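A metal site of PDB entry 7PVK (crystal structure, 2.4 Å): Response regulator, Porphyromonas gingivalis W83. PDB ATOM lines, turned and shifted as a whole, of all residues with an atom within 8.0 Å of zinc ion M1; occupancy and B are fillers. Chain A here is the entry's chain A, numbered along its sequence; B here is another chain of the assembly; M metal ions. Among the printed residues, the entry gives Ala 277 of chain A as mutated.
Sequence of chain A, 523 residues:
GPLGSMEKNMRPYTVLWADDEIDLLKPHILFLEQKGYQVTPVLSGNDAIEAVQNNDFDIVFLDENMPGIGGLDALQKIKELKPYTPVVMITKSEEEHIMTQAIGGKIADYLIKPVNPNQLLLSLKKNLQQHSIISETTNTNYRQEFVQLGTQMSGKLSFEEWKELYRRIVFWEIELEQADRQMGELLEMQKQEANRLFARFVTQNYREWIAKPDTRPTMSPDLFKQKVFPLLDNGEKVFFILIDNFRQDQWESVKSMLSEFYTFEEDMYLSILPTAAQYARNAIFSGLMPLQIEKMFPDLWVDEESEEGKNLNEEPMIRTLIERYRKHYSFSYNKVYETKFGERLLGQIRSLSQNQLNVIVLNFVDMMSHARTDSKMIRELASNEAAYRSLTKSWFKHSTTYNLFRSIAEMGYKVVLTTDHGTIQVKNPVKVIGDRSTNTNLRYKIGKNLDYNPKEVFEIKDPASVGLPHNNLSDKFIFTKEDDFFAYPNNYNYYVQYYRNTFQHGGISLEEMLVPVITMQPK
The side-chain carboxylate (OD1) of Asp 366 sits close to the side-chain amide nitrogen (ND2) of Asn 245 (3.5 Å). A ring nitrogen (ND1) of His 505 sits at hydrogen-bond distance from the backbone carbonyl oxygen (O) of Thr 275 (2.8 Å). The backbone NH (N) of Ala 277 is in hydrogen-bond range of OP1 of G 1 of chain B. N of Asp 366 lies within hydrogen-bond range of O of Asp 244, 3.3 Å away. O of His 505 sits at hydrogen-bond distance from ND2 of Asn 441 (3.3 Å). A ring nitrogen (ND1) of His 505 sits close to a ring nitrogen (ND1) of His 421 (3.5 Å).
Within 4 Å of zinc ion M1: Asp 366, His 370, His 505 and G 1 of chain B. Along chain A the residues within 4 Å of zinc ion M1 span positions 366 to 505.
OD1 of Asp 366 binds zinc ion M1 (1.7 Å). A ring nitrogen (NE2) of His 505 binds zinc ion M1 (2.0 Å). NE2 of His 370 binds zinc ion M1 (2.0 Å). Zinc ion M1 is bound by OP2 of G 1 of chain B (2.0 Å).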
ATOM      1  N   ASP A 244      -3.248  18.491  16.707  1.00  0.00           N
ATOM      2  CA  ASP A 244      -3.092  17.203  16.055  1.00  0.00           C
ATOM      3  C   ASP A 244      -3.992  17.118  14.838  1.00  0.00           C
ATOM      4  O   ASP A 244      -5.176  17.469  14.897  1.00  0.00           O
ATOM      5  CB  ASP A 244      -3.412  16.079  17.043  1.00  0.00           C
ATOM      6  CG  ASP A 244      -2.847  14.742  16.600  1.00  0.00           C
ATOM      7  OD1 ASP A 244      -3.081  14.362  15.436  1.00  0.00           O
ATOM      8  OD2 ASP A 244      -2.148  14.092  17.411  1.00  0.00           O
ATOM      9  N   ASN A 245      -3.422  16.657  13.726  1.00  0.00           N
ATOM     10  CA  ASN A 245      -4.171  16.414  12.500  1.00  0.00           C
ATOM     11  C   ASN A 245      -4.679  17.726  11.908  1.00  0.00           C
ATOM     12  O   ASN A 245      -5.887  17.914  11.733  1.00  0.00           O
ATOM     13  CB  ASN A 245      -5.341  15.463  12.779  1.00  0.00           C
ATOM     14  CG  ASN A 245      -5.757  14.697  11.543  1.00  0.00           C
ATOM     15  OD1 ASN A 245      -5.569  15.153  10.418  1.00  0.00           O
ATOM     16  ND2 ASN A 245      -6.339  13.518  11.747  1.00  0.00           N
ATOM     17  N   THR A 275       2.564   8.493   9.445  1.00  0.00           N
ATOM     18  CA  THR A 275       2.053   9.817   9.805  1.00  0.00           C
ATOM     19  C   THR A 275       0.978   9.658  10.872  1.00  0.00           C
ATOM     20  O   THR A 275      -0.235   9.701  10.616  1.00  0.00           O
ATOM     21  CB  THR A 275       1.515  10.530   8.560  1.00  0.00           C
ATOM     22  OG1 THR A 275       0.701   9.619   7.812  1.00  0.00           O
ATOM     23  CG2 THR A 275       2.667  11.015   7.706  1.00  0.00           C
ATOM     24  N   ALA A 276       1.434   9.448  12.101  1.00  0.00           N
ATOM     25  CA  ALA A 276       0.563   9.318  13.260  1.00  0.00           C
ATOM     26  C   ALA A 276       1.319   9.809  14.488  1.00  0.00           C
ATOM     27  O   ALA A 276       2.548   9.936  14.476  1.00  0.00           O
ATOM     28  CB  ALA A 276       0.093   7.870  13.448  1.00  0.00           C
ATOM     29  N   ALA A 277       0.573  10.095  15.554  1.00  0.00           N
ATOM     30  CA  ALA A 277       1.170  10.703  16.732  1.00  0.00           C
ATOM     31  C   ALA A 277       2.190   9.794  17.406  1.00  0.00           C
ATOM     32  O   ALA A 277       3.166  10.283  17.981  1.00  0.00           O
ATOM     33  CB  ALA A 277       0.068  11.075  17.731  1.00  0.00           C
ATOM     34  N   ASN A 363      -6.256  18.189  20.708  1.00  0.00           N
ATOM     35  CA  ASN A 363      -6.563  16.927  20.043  1.00  0.00           C
ATOM     36  C   ASN A 363      -7.937  16.867  19.399  1.00  0.00           C
ATOM     37  O   ASN A 363      -8.236  15.870  18.732  1.00  0.00           O
ATOM     38  CB  ASN A 363      -6.450  15.762  21.050  1.00  0.00           C
ATOM     39  CG  ASN A 363      -5.009  15.428  21.393  1.00  0.00           C
ATOM     40  OD1 ASN A 363      -4.211  15.132  20.503  1.00  0.00           O
ATOM     41  ND2 ASN A 363      -4.684  15.462  22.683  1.00  0.00           N
ATOM     42  N   VAL A 365      -9.286  18.200  16.826  1.00  0.00           N
ATOM     43  CA  VAL A 365      -9.313  18.091  15.369  1.00  0.00           C
ATOM     44  C   VAL A 365      -9.017  16.667  14.936  1.00  0.00           C
ATOM     45  O   VAL A 365      -9.612  16.150  13.983  1.00  0.00           O
ATOM     46  CB  VAL A 365      -8.339  19.091  14.739  1.00  0.00           C
ATOM     47  CG1 VAL A 365      -8.346  18.973  13.215  1.00  0.00           C
ATOM     48  CG2 VAL A 365      -8.701  20.521  15.149  1.00  0.00           C
ATOM     49  N   ASP A 366      -8.083  15.991  15.630  1.00  0.00           N
ATOM     50  CA  ASP A 366      -7.845  14.578  15.327  1.00  0.00           C
ATOM     51  C   ASP A 366      -9.050  13.736  15.732  1.00  0.00           C
ATOM     52  O   ASP A 366      -9.442  12.829  14.988  1.00  0.00           O
ATOM     53  CB  ASP A 366      -6.580  14.101  16.027  1.00  0.00           C
ATOM     54  CG  ASP A 366      -6.374  12.600  15.896  1.00  0.00           C
ATOM     55  OD1 ASP A 366      -5.762  12.159  14.900  1.00  0.00           O
ATOM     56  OD2 ASP A 366      -6.858  11.862  16.787  1.00  0.00           O
ATOM     57  N   MET A 367      -9.637  14.024  16.883  1.00  0.00           N
ATOM     58  CA  MET A 367     -10.825  13.322  17.344  1.00  0.00           C
ATOM     59  C   MET A 367     -11.958  13.456  16.321  1.00  0.00           C
ATOM     60  O   MET A 367     -12.671  12.491  16.048  1.00  0.00           O
ATOM     61  CB  MET A 367     -11.278  13.860  18.704  1.00  0.00           C
ATOM     62  CG  MET A 367     -10.246  13.686  19.817  1.00  0.00           C
ATOM     63  SD  MET A 367     -10.558  14.828  21.380  1.00  0.00           S
ATOM     64  CE  MET A 367     -12.256  14.084  21.979  1.00  0.00           C
ATOM     65  N   MET A 368     -12.096  14.649  15.754  1.00  0.00           N
ATOM     66  CA  MET A 368     -13.142  14.927  14.769  1.00  0.00           C
ATOM     67  C   MET A 368     -12.831  14.268  13.444  1.00  0.00           C
ATOM     68  O   MET A 368     -13.700  13.656  12.817  1.00  0.00           O
ATOM     69  CB  MET A 368     -13.309  16.431  14.570  1.00  0.00           C
ATOM     70  CG  MET A 368     -14.439  16.790  13.616  1.00  0.00           C
ATOM     71  SD  MET A 368     -13.846  17.271  11.820  1.00  0.00           S
ATOM     72  CE  MET A 368     -13.288  19.105  12.176  1.00  0.00           C
ATOM     73  N   SER A 369     -11.574  14.407  12.991  1.00  0.00           N
ATOM     74  CA  SER A 369     -11.153  13.749  11.762  1.00  0.00           C
ATOM     75  C   SER A 369     -11.419  12.252  11.831  1.00  0.00           C
ATOM     76  O   SER A 369     -11.814  11.641  10.822  1.00  0.00           O
ATOM     77  CB  SER A 369      -9.681  14.030  11.500  1.00  0.00           C
ATOM     78  OG  SER A 369      -9.226  13.323  10.360  1.00  0.00           O
ATOM     79  N   HIS A 370     -11.203  11.637  12.990  1.00  0.00           N
ATOM     80  CA  HIS A 370     -11.497  10.222  13.139  1.00  0.00           C
ATOM     81  C   HIS A 370     -12.996   9.971  13.185  1.00  0.00           C
ATOM     82  O   HIS A 370     -13.482   8.974  12.641  1.00  0.00           O
ATOM     83  CB  HIS A 370     -10.842   9.684  14.411  1.00  0.00           C
ATOM     84  CG  HIS A 370      -9.360   9.484  14.285  1.00  0.00           C
ATOM     85  ND1 HIS A 370      -8.802   8.555  13.430  1.00  0.00           N
ATOM     86  CD2 HIS A 370      -8.327  10.102  14.904  1.00  0.00           C
ATOM     87  CE1 HIS A 370      -7.489   8.612  13.534  1.00  0.00           C
ATOM     88  NE2 HIS A 370      -7.174   9.534  14.422  1.00  0.00           N
ATOM     89  N   ASP A 420       1.410  17.498  13.927  1.00  0.00           N
ATOM     90  CA  ASP A 420       2.217  16.291  13.799  1.00  0.00           C
ATOM     91  C   ASP A 420       1.982  15.532  12.507  1.00  0.00           C
ATOM     92  O   ASP A 420       2.825  14.714  12.125  1.00  0.00           O
ATOM     93  CB  ASP A 420       1.937  15.339  14.979  1.00  0.00           C
ATOM     94  CG  ASP A 420       0.483  14.955  15.084  1.00  0.00           C
ATOM     95  OD1 ASP A 420      -0.388  15.714  14.597  1.00  0.00           O
ATOM     96  OD2 ASP A 420       0.194  13.874  15.641  1.00  0.00           O
ATOM     97  N   HIS A 421       0.864  15.780  11.829  1.00  0.00           N
ATOM     98  CA  HIS A 421       0.539  15.088  10.584  1.00  0.00           C
ATOM     99  C   HIS A 421      -0.768  15.683  10.076  1.00  0.00           C
ATOM    100  O   HIS A 421      -1.479  16.393  10.793  1.00  0.00           O
ATOM    101  CB  HIS A 421       0.400  13.585  10.782  1.00  0.00           C
ATOM    102  CG  HIS A 421      -0.675  13.201  11.750  1.00  0.00           C
ATOM    103  ND1 HIS A 421      -2.010  13.164  11.411  1.00  0.00           N
ATOM    104  CD2 HIS A 421      -0.608  12.842  13.061  1.00  0.00           C
ATOM    105  CE1 HIS A 421      -2.718  12.797  12.466  1.00  0.00           C
ATOM    106  NE2 HIS A 421      -1.898  12.592  13.476  1.00  0.00           N
ATOM    107  N   GLY A 422      -1.069  15.393   8.815  1.00  0.00           N
ATOM    108  CA  GLY A 422      -2.327  15.743   8.217  1.00  0.00           C
ATOM    109  C   GLY A 422      -3.273  14.560   8.142  1.00  0.00           C
ATOM    110  O   GLY A 422      -3.227  13.651   8.984  1.00  0.00           O
ATOM    111  N   THR A 423      -4.142  14.582   7.144  1.00  0.00           N
ATOM    112  CA  THR A 423      -5.020  13.449   6.859  1.00  0.00           C
ATOM    113  C   THR A 423      -5.547  13.622   5.449  1.00  0.00           C
ATOM    114  O   THR A 423      -5.569  14.723   4.899  1.00  0.00           O
ATOM    115  CB  THR A 423      -6.174  13.353   7.861  1.00  0.00           C
ATOM    116  OG1 THR A 423      -6.690  12.013   7.871  1.00  0.00           O
ATOM    117  CG2 THR A 423      -7.312  14.324   7.525  1.00  0.00           C
ATOM    118  N   ASN A 441      -4.738   0.389  11.875  1.00  0.00           N
ATOM    119  CA  ASN A 441      -4.631   1.581  11.046  1.00  0.00           C
ATOM    120  C   ASN A 441      -4.789   1.200   9.576  1.00  0.00           C
ATOM    121  O   ASN A 441      -4.366   0.121   9.139  1.00  0.00           O
ATOM    122  CB  ASN A 441      -3.276   2.266  11.272  1.00  0.00           C
ATOM    123  CG  ASN A 441      -3.140   3.563  10.503  1.00  0.00           C
ATOM    124  OD1 ASN A 441      -3.324   3.604   9.283  1.00  0.00           O
ATOM    125  ND2 ASN A 441      -2.831   4.627  11.214  1.00  0.00           N
ATOM    126  N   PHE A 503     -11.484  10.134   6.340  1.00  0.00           N
ATOM    127  CA  PHE A 503     -10.166  10.735   6.545  1.00  0.00           C
ATOM    128  C   PHE A 503      -9.292   9.755   7.319  1.00  0.00           C
ATOM    129  O   PHE A 503      -9.671   9.283   8.394  1.00  0.00           O
ATOM    130  CB  PHE A 503     -10.290  12.062   7.281  1.00  0.00           C
ATOM    131  CG  PHE A 503     -11.113  13.089   6.550  1.00  0.00           C
ATOM    132  CD1 PHE A 503     -10.769  13.474   5.266  1.00  0.00           C
ATOM    133  CD2 PHE A 503     -12.218  13.665   7.147  1.00  0.00           C
ATOM    134  CE1 PHE A 503     -11.522  14.420   4.592  1.00  0.00           C
ATOM    135  CE2 PHE A 503     -12.971  14.610   6.473  1.00  0.00           C
ATOM    136  CZ  PHE A 503     -12.627  14.986   5.199  1.00  0.00           C
ATOM    137  N   GLN A 504      -8.119   9.441   6.757  1.00  0.00           N
ATOM    138  CA  GLN A 504      -7.193   8.508   7.370  1.00  0.00           C
ATOM    139  C   GLN A 504      -5.785   9.060   7.231  1.00  0.00           C
ATOM    140  O   GLN A 504      -5.410   9.551   6.165  1.00  0.00           O
ATOM    141  CB  GLN A 504      -7.271   7.125   6.731  1.00  0.00           C
ATOM    142  CG  GLN A 504      -8.661   6.512   6.742  1.00  0.00           C
ATOM    143  CD  GLN A 504      -9.186   6.297   8.145  1.00  0.00           C
ATOM    144  OE1 GLN A 504      -8.435   6.353   9.113  1.00  0.00           O
ATOM    145  NE2 GLN A 504     -10.492   6.059   8.258  1.00  0.00           N
ATOM    146  N   HIS A 505      -5.008   8.957   8.302  1.00  0.00           N
ATOM    147  CA  HIS A 505      -3.608   9.336   8.301  1.00  0.00           C
ATOM    148  C   HIS A 505      -2.757   8.130   8.674  1.00  0.00           C
ATOM    149  O   HIS A 505      -3.266   7.102   9.130  1.00  0.00           O
ATOM    150  CB  HIS A 505      -3.344  10.515   9.251  1.00  0.00           C
ATOM    151  CG  HIS A 505      -3.737  10.240  10.662  1.00  0.00           C
ATOM    152  ND1 HIS A 505      -2.841   9.820  11.621  1.00  0.00           N
ATOM    153  CD2 HIS A 505      -4.935  10.339  11.293  1.00  0.00           C
ATOM    154  CE1 HIS A 505      -3.463   9.679  12.774  1.00  0.00           C
ATOM    155  NE2 HIS A 505      -4.740   9.978  12.598  1.00  0.00           N
ATOM    156  N   GLY A 506      -1.453   8.274   8.470  1.00  0.00           N
ATOM    157  CA  GLY A 506      -0.500   7.201   8.684  1.00  0.00           C
ATOM    158  C   GLY A 506       0.268   6.802   7.440  1.00  0.00           C
ATOM    159  O   GLY A 506       1.333   6.173   7.549  1.00  0.00           O
ATOM    160  P     G B   1      -3.156  10.031  16.172  1.00  0.00           P
ATOM    161  OP1   G B   1      -2.093   9.188  15.586  1.00  0.00           O
ATOM    162  OP2   G B   1      -4.458   9.512  15.703  1.00  0.00           O
ATOM    163  O5'   G B   1      -3.149   9.839  17.743  1.00  0.00           O
ATOM    164  C5'   G B   1      -4.086  10.537  18.560  1.00  0.00           C
ATOM    165  C4'   G B   1      -3.987  10.117  20.018  1.00  0.00           C
ATOM    166  O4'   G B   1      -4.487   8.756  20.134  1.00  0.00           O
ATOM    167  C3'   G B   1      -2.567  10.124  20.591  1.00  0.00           C
ATOM    168  O3'   G B   1      -2.506  10.583  21.952  1.00  0.00           O
ATOM    169  C2'   G B   1      -2.174   8.639  20.539  1.00  0.00           C
ATOM    170  O2'   G B   1      -1.236   8.256  21.523  1.00  0.00           O
ATOM    171  C1'   G B   1      -3.518   7.955  20.776  1.00  0.00           C
ATOM    172  N9    G B   1      -3.592   6.596  20.227  1.00  0.00           N
ATOM    173  C8    G B   1      -3.362   6.219  18.929  1.00  0.00           C
ATOM    174  N7    G B   1      -3.501   4.934  18.738  1.00  0.00           N
ATOM    175  C5    G B   1      -3.850   4.442  19.989  1.00  0.00           C
ATOM    176  C6    G B   1      -4.138   3.111  20.414  1.00  0.00           C
ATOM    177  O6    G B   1      -4.147   2.073  19.751  1.00  0.00           O
ATOM    178  N1    G B   1      -4.447   3.069  21.771  1.00  0.00           N
ATOM    179  C2    G B   1      -4.473   4.143  22.608  1.00  0.00           C
ATOM    180  N2    G B   1      -4.799   3.903  23.883  1.00  0.00           N
ATOM    181  N3    G B   1      -4.209   5.391  22.231  1.00  0.00           N
ATOM    182  C4    G B   1      -3.908   5.461  20.919  1.00  0.00           C
ATOM    183  P     G B   2      -3.593  11.569  22.598  1.00  0.00           P
ATOM    184  OP1   G B   2      -4.117  12.521  21.583  1.00  0.00           O
ATOM    185  OP2   G B   2      -2.973  12.138  23.827  1.00  0.00           O
ATOM    186  O5'   G B   2      -4.727  10.558  23.065  1.00  0.00           O
ATOM    187  C5'   G B   2      -6.086  10.957  23.193  1.00  0.00           C
ATOM    188  C4'   G B   2      -6.799  10.126  24.225  1.00  0.00           C
ATOM    189  O4'   G B   2      -5.882   9.869  25.330  1.00  0.00           O
ATOM    190  C3'   G B   2      -8.040  10.762  24.843  1.00  0.00           C
ATOM    191  O3'   G B   2      -9.011   9.762  25.150  1.00  0.00           O
ATOM    192  C2'   G B   2      -7.509  11.380  26.140  1.00  0.00           C
ATOM    193  O2'   G B   2      -8.487  11.505  27.154  1.00  0.00           O
ATOM    194  C1'   G B   2      -6.416  10.383  26.541  1.00  0.00           C
ATOM    195  N9    G B   2      -5.314  10.982  27.298  1.00  0.00           N
ATOM    196  C8    G B   2      -4.145  11.462  26.753  1.00  0.00           C
ATOM    197  N7    G B   2      -3.317  11.941  27.644  1.00  0.00           N
ATOM    198  C5    G B   2      -3.961  11.741  28.849  1.00  0.00           C
ATOM    199  C6    G B   2      -3.544  12.064  30.170  1.00  0.00           C
ATOM    200  O6    G B   2      -2.488  12.584  30.537  1.00  0.00           O
ATOM    201  N1    G B   2      -4.499  11.702  31.107  1.00  0.00           N
ATOM    202  C2    G B   2      -5.703  11.113  30.824  1.00  0.00           C
ATOM    203  N2    G B   2      -6.481  10.840  31.882  1.00  0.00           N
ATOM    204  N3    G B   2      -6.108  10.808  29.599  1.00  0.00           N
ATOM    205  C4    G B   2      -5.191  11.145  28.667  1.00  0.00           C
HETATM  206 ZN    ZN M   1      -5.473  10.560  14.330  1.00  0.00          ZN
HETATM  207 ZN    ZN M   2      -1.797  13.003  15.348  1.00  0.00          ZN
